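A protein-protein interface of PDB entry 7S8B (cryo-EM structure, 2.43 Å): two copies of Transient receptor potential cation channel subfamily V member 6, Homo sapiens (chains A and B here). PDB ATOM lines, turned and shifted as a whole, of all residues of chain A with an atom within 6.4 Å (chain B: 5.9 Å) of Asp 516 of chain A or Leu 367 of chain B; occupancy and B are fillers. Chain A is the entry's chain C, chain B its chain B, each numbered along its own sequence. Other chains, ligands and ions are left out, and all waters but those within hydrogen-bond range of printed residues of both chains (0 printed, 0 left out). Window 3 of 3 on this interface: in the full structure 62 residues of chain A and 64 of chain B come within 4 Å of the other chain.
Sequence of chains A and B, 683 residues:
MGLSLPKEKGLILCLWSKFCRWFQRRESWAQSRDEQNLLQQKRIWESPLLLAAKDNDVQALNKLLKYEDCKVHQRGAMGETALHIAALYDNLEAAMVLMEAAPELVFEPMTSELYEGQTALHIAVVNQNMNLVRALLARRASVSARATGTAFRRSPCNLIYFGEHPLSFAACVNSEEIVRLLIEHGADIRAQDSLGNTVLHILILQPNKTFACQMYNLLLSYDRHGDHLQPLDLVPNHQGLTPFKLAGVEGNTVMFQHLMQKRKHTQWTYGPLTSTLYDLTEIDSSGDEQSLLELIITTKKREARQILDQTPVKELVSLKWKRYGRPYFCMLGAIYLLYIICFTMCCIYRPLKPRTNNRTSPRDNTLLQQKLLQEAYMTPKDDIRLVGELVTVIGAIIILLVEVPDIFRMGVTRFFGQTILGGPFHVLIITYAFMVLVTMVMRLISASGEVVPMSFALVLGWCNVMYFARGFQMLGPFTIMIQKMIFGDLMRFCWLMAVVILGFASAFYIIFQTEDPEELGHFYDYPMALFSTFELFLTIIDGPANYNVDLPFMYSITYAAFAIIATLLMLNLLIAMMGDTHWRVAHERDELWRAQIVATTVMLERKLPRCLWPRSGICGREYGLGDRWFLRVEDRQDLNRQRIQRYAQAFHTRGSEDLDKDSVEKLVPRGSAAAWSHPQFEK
The backbone NH (N) of Leu 367 of chain B is in hydrogen-bond range of the backbone carbonyl oxygen (O) of Thr 514 of chain A, 2.7 Å away.
The backbone carbonyl oxygen of Asn 365 of chain B lies within hydrogen-bond range of the backbone NH of Asp 516 of chain A (3.0 Å).
O of Thr 514 of chain A lies within hydrogen-bond range of N of Leu 368 of chain B (3.2 Å).
OE1 of Glu 519 of chain A is in hydrogen-bond range of ND2 of Asn 365 of chain B, at 2.4 Å.
No position is printed for both chains.
N of Arg 355 of chain B is in hydrogen-bond range of O of Leu 367 of chain B.
O of Thr 366 of chain B sits at hydrogen-bond distance from NH2 of Arg 355 of chain B, at 2.8 Å.
The side-chain hydroxyl (OG1) of Thr 514 of chain A sits at hydrogen-bond distance from the side-chain carboxylate (OE2) of Glu 515 of chain A, 3.4 Å away.
The side-chain carboxylate (OD1) of Asp 516 of chain A lies close to the backbone NH (N) of Glu 518 of chain A (3.2 Å).
Hydrophobic or aromatic side chains of chain B within 4 Å of the printed part of chain A: Leu 367 and Leu 368.
Along chain B the printed residues that touch a printed residue of chain A span positions 365 to 368.
Of the 9 printed residues of chain A, 4 touch a printed residue of chain B.
Along chain A the printed residues that touch a printed residue of chain B span positions 514 to 519.
Among the printed residues, 9 pairs touch across the chains.
Among the printed residues, no Asp or Glu carboxylate lies within 4 Å of a Lys or Arg side-chain nitrogen of the other chain.
Printed residues of chain B within 4 Å of Asp 516 of chain A: Asn 365 (3.0 Å) and Leu 367 (3.8 Å).
Leu 367 of chain B touches just these residues of chain A: Thr 514 (2.7 Å), Glu 515 (3.7 Å) and Asp 516 (3.8 Å).
Of the printed residues of chain B, Thr 514 of chain A touches Thr 366, Leu 367 and Leu 368.
Printed residues of chain B within 4 Å of Glu 515 of chain A: Asn 365, Thr 366 and Leu 367.
Of the printed residues of chain A, Asn 365 of chain B touches Glu 515, Asp 516 and Glu 519.
Of the printed residues of chain A, Leu 368 of chain B touches Thr 514 (3.2 Å).
Of the printed residues of chain A, Thr 366 of chain B touches Thr 514 and Glu 515.
Glu 518 of chain A touches none of the printed residues of chain B.
The nearest residue of chain A that does not touch Leu 367 of chain B is Pro 517 of chain A (4.4 Å).
Thr 514 of chain A touches Thr 366 of chain B.
Glu 515 of chain A touches Asn 365 of chain B.
Glu 515 of chain A touches Thr 366 of chain B.
Leu 367 of chain B touches Glu 515 of chain A.
Leu 367 of chain B touches Asp 516 of chain A (CD1 to CA, 3.8 Å).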
ATOM      1  N   PHE A 512      38.032  -4.534  -8.245  1.00  0.00           N
ATOM      2  CA  PHE A 512      36.816  -4.827  -8.983  1.00  0.00           C
ATOM      3  C   PHE A 512      36.124  -6.097  -8.511  1.00  0.00           C
ATOM      4  O   PHE A 512      35.209  -6.575  -9.182  1.00  0.00           O
ATOM      5  CB  PHE A 512      37.128  -4.910 -10.476  1.00  0.00           C
ATOM      6  CG  PHE A 512      37.444  -3.589 -11.082  1.00  0.00           C
ATOM      7  CD1 PHE A 512      36.431  -2.746 -11.472  1.00  0.00           C
ATOM      8  CD2 PHE A 512      38.744  -3.163 -11.212  1.00  0.00           C
ATOM      9  CE1 PHE A 512      36.709  -1.515 -12.010  1.00  0.00           C
ATOM     10  CE2 PHE A 512      39.029  -1.949 -11.754  1.00  0.00           C
ATOM     11  CZ  PHE A 512      38.017  -1.121 -12.153  1.00  0.00           C
ATOM     12  N   THR A 514      34.182  -6.481  -5.948  1.00  0.00           N
ATOM     13  CA  THR A 514      32.851  -6.155  -5.463  1.00  0.00           C
ATOM     14  C   THR A 514      31.974  -5.474  -6.504  1.00  0.00           C
ATOM     15  O   THR A 514      30.876  -5.029  -6.167  1.00  0.00           O
ATOM     16  CB  THR A 514      32.941  -5.256  -4.229  1.00  0.00           C
ATOM     17  OG1 THR A 514      33.711  -4.090  -4.532  1.00  0.00           O
ATOM     18  CG2 THR A 514      33.568  -5.982  -3.079  1.00  0.00           C
ATOM     19  N   GLU A 515      32.424  -5.369  -7.747  1.00  0.00           N
ATOM     20  CA  GLU A 515      31.693  -4.646  -8.771  1.00  0.00           C
ATOM     21  C   GLU A 515      30.889  -5.621  -9.619  1.00  0.00           C
ATOM     22  O   GLU A 515      30.920  -6.833  -9.421  1.00  0.00           O
ATOM     23  CB  GLU A 515      32.648  -3.828  -9.645  1.00  0.00           C
ATOM     24  CG  GLU A 515      33.580  -2.943  -8.862  1.00  0.00           C
ATOM     25  CD  GLU A 515      32.870  -1.905  -8.034  1.00  0.00           C
ATOM     26  OE1 GLU A 515      31.871  -1.332  -8.495  1.00  0.00           O
ATOM     27  OE2 GLU A 515      33.304  -1.677  -6.889  1.00  0.00           O
ATOM     28  N   ASP A 516      30.146  -5.073 -10.570  1.00  0.00           N
ATOM     29  CA  ASP A 516      29.446  -5.878 -11.558  1.00  0.00           C
ATOM     30  C   ASP A 516      30.341  -6.040 -12.776  1.00  0.00           C
ATOM     31  O   ASP A 516      30.682  -5.038 -13.412  1.00  0.00           O
ATOM     32  CB  ASP A 516      28.129  -5.218 -11.934  1.00  0.00           C
ATOM     33  CG  ASP A 516      27.216  -6.102 -12.780  1.00  0.00           C
ATOM     34  OD1 ASP A 516      27.582  -7.222 -13.169  1.00  0.00           O
ATOM     35  OD2 ASP A 516      26.089  -5.662 -13.054  1.00  0.00           O
ATOM     36  N   PRO A 517      30.745  -7.262 -13.135  1.00  0.00           N
ATOM     37  CA  PRO A 517      31.641  -7.438 -14.285  1.00  0.00           C
ATOM     38  C   PRO A 517      30.968  -7.244 -15.625  1.00  0.00           C
ATOM     39  O   PRO A 517      31.671  -7.173 -16.636  1.00  0.00           O
ATOM     40  CB  PRO A 517      32.131  -8.879 -14.125  1.00  0.00           C
ATOM     41  CG  PRO A 517      31.044  -9.544 -13.401  1.00  0.00           C
ATOM     42  CD  PRO A 517      30.469  -8.540 -12.463  1.00  0.00           C
ATOM     43  N   GLU A 518      29.638  -7.175 -15.670  1.00  0.00           N
ATOM     44  CA  GLU A 518      28.928  -6.938 -16.921  1.00  0.00           C
ATOM     45  C   GLU A 518      29.246  -5.570 -17.491  1.00  0.00           C
ATOM     46  O   GLU A 518      29.238  -5.380 -18.711  1.00  0.00           O
ATOM     47  CB  GLU A 518      27.431  -7.081 -16.680  1.00  0.00           C
ATOM     48  CG  GLU A 518      27.058  -8.498 -16.316  1.00  0.00           C
ATOM     49  CD  GLU A 518      27.176  -9.420 -17.500  1.00  0.00           C
ATOM     50  OE1 GLU A 518      26.768  -9.003 -18.603  1.00  0.00           O
ATOM     51  OE2 GLU A 518      27.721 -10.531 -17.349  1.00  0.00           O
ATOM     52  N   GLU A 519      29.560  -4.619 -16.627  1.00  0.00           N
ATOM     53  CA  GLU A 519      29.894  -3.278 -17.048  1.00  0.00           C
ATOM     54  C   GLU A 519      31.394  -3.049 -17.174  1.00  0.00           C
ATOM     55  O   GLU A 519      31.801  -2.121 -17.880  1.00  0.00           O
ATOM     56  CB  GLU A 519      29.248  -2.294 -16.070  1.00  0.00           C
ATOM     57  CG  GLU A 519      27.718  -2.342 -16.211  1.00  0.00           C
ATOM     58  CD  GLU A 519      26.988  -1.544 -15.164  1.00  0.00           C
ATOM     59  OE1 GLU A 519      27.651  -1.055 -14.236  1.00  0.00           O
ATOM     60  OE2 GLU A 519      25.753  -1.413 -15.260  1.00  0.00           O
ATOM     61  N   LEU A 520      32.217  -3.891 -16.541  1.00  0.00           N
ATOM     62  CA  LEU A 520      33.669  -3.830 -16.707  1.00  0.00           C
ATOM     63  C   LEU A 520      34.227  -5.207 -16.349  1.00  0.00           C
ATOM     64  O   LEU A 520      34.355  -5.531 -15.171  1.00  0.00           O
ATOM     65  CB  LEU A 520      34.267  -2.737 -15.842  1.00  0.00           C
ATOM     66  CG  LEU A 520      35.684  -2.306 -16.178  1.00  0.00           C
ATOM     67  CD1 LEU A 520      35.724  -0.846 -15.969  1.00  0.00           C
ATOM     68  CD2 LEU A 520      36.718  -3.003 -15.314  1.00  0.00           C
ATOM     69  N   GLY A 521      34.567  -5.993 -17.366  1.00  0.00           N
ATOM     70  CA  GLY A 521      34.884  -7.390 -17.176  1.00  0.00           C
ATOM     71  C   GLY A 521      36.337  -7.778 -17.281  1.00  0.00           C
ATOM     72  O   GLY A 521      36.632  -8.979 -17.309  1.00  0.00           O
ATOM     73  N   LYS B 353      30.236 -10.605   0.738  1.00  0.00           N
ATOM     74  CA  LYS B 353      28.859 -11.072   0.744  1.00  0.00           C
ATOM     75  C   LYS B 353      28.052 -10.194  -0.186  1.00  0.00           C
ATOM     76  O   LYS B 353      28.489  -9.087  -0.533  1.00  0.00           O
ATOM     77  CB  LYS B 353      28.270 -11.040   2.162  1.00  0.00           C
ATOM     78  CG  LYS B 353      28.120  -9.669   2.739  1.00  0.00           C
ATOM     79  CD  LYS B 353      27.527  -9.751   4.115  1.00  0.00           C
ATOM     80  CE  LYS B 353      27.368  -8.389   4.726  1.00  0.00           C
ATOM     81  NZ  LYS B 353      26.754  -8.490   6.070  1.00  0.00           N
ATOM     82  N   PRO B 354      26.881 -10.659  -0.656  1.00  0.00           N
ATOM     83  CA  PRO B 354      25.987  -9.786  -1.425  1.00  0.00           C
ATOM     84  C   PRO B 354      25.544  -8.561  -0.643  1.00  0.00           C
ATOM     85  O   PRO B 354      25.375  -8.606   0.574  1.00  0.00           O
ATOM     86  CB  PRO B 354      24.801 -10.694  -1.753  1.00  0.00           C
ATOM     87  CG  PRO B 354      25.380 -12.032  -1.783  1.00  0.00           C
ATOM     88  CD  PRO B 354      26.427 -12.063  -0.718  1.00  0.00           C
ATOM     89  N   ARG B 355      25.381  -7.455  -1.363  1.00  0.00           N
ATOM     90  CA  ARG B 355      25.077  -6.176  -0.737  1.00  0.00           C
ATOM     91  C   ARG B 355      23.676  -6.176  -0.133  1.00  0.00           C
ATOM     92  O   ARG B 355      22.766  -6.867  -0.602  1.00  0.00           O
ATOM     93  CB  ARG B 355      25.212  -5.036  -1.748  1.00  0.00           C
ATOM     94  CG  ARG B 355      24.210  -5.074  -2.876  1.00  0.00           C
ATOM     95  CD  ARG B 355      24.396  -3.888  -3.763  1.00  0.00           C
ATOM     96  NE  ARG B 355      24.243  -2.645  -3.015  1.00  0.00           N
ATOM     97  CZ  ARG B 355      24.658  -1.464  -3.458  1.00  0.00           C
ATOM     98  NH1 ARG B 355      24.499  -0.376  -2.721  1.00  0.00           N
ATOM     99  NH2 ARG B 355      25.231  -1.375  -4.644  1.00  0.00           N
ATOM    100  N   ASN B 365      27.634   0.622  -9.200  1.00  0.00           N
ATOM    101  CA  ASN B 365      28.071  -0.611  -9.828  1.00  0.00           C
ATOM    102  C   ASN B 365      28.289  -1.737  -8.837  1.00  0.00           C
ATOM    103  O   ASN B 365      28.552  -2.865  -9.255  1.00  0.00           O
ATOM    104  CB  ASN B 365      29.388  -0.388 -10.579  1.00  0.00           C
ATOM    105  CG  ASN B 365      29.533  -1.280 -11.782  1.00  0.00           C
ATOM    106  OD1 ASN B 365      30.566  -1.292 -12.436  1.00  0.00           O
ATOM    107  ND2 ASN B 365      28.459  -1.953 -12.141  1.00  0.00           N
ATOM    108  N   THR B 366      28.207  -1.451  -7.547  1.00  0.00           N
ATOM    109  CA  THR B 366      28.633  -2.381  -6.517  1.00  0.00           C
ATOM    110  C   THR B 366      27.647  -3.535  -6.378  1.00  0.00           C
ATOM    111  O   THR B 366      26.442  -3.321  -6.240  1.00  0.00           O
ATOM    112  CB  THR B 366      28.754  -1.631  -5.198  1.00  0.00           C
ATOM    113  OG1 THR B 366      29.621  -0.506  -5.362  1.00  0.00           O
ATOM    114  CG2 THR B 366      29.326  -2.508  -4.165  1.00  0.00           C
ATOM    115  N   LEU B 367      28.156  -4.759  -6.426  1.00  0.00           N
ATOM    116  CA  LEU B 367      27.330  -5.925  -6.161  1.00  0.00           C
ATOM    117  C   LEU B 367      27.533  -6.485  -4.768  1.00  0.00           C
ATOM    118  O   LEU B 367      26.603  -7.058  -4.199  1.00  0.00           O
ATOM    119  CB  LEU B 367      27.626  -7.037  -7.170  1.00  0.00           C
ATOM    120  CG  LEU B 367      27.051  -6.921  -8.571  1.00  0.00           C
ATOM    121  CD1 LEU B 367      27.424  -8.156  -9.343  1.00  0.00           C
ATOM    122  CD2 LEU B 367      25.562  -6.771  -8.527  1.00  0.00           C
ATOM    123  N   LEU B 368      28.722  -6.320  -4.208  1.00  0.00           N
ATOM    124  CA  LEU B 368      29.163  -7.076  -3.053  1.00  0.00           C
ATOM    125  C   LEU B 368      29.709  -6.117  -2.017  1.00  0.00           C
ATOM    126  O   LEU B 368      30.195  -5.038  -2.346  1.00  0.00           O
ATOM    127  CB  LEU B 368      30.261  -8.067  -3.428  1.00  0.00           C
ATOM    128  CG  LEU B 368      29.873  -9.219  -4.339  1.00  0.00           C
ATOM    129  CD1 LEU B 368      31.096 -10.023  -4.677  1.00  0.00           C
ATOM    130  CD2 LEU B 368      28.833 -10.085  -3.705  1.00  0.00           C
ATOM    131  N   GLN B 369      29.638  -6.512  -0.763  1.00  0.00           N
ATOM    132  CA  GLN B 369      30.323  -5.785   0.283  1.00  0.00           C
ATOM    133  C   GLN B 369      31.016  -6.793   1.178  1.00  0.00           C
ATOM    134  O   GLN B 369      30.765  -7.998   1.105  1.00  0.00           O
ATOM    135  CB  GLN B 369      29.370  -4.897   1.082  1.00  0.00           C
ATOM    136  CG  GLN B 369      28.296  -5.662   1.773  1.00  0.00           C
ATOM    137  CD  GLN B 369      27.425  -4.785   2.623  1.00  0.00           C
ATOM    138  OE1 GLN B 369      27.674  -3.591   2.769  1.00  0.00           O
ATOM    139  NE2 GLN B 369      26.400  -5.371   3.197  1.00  0.00           N
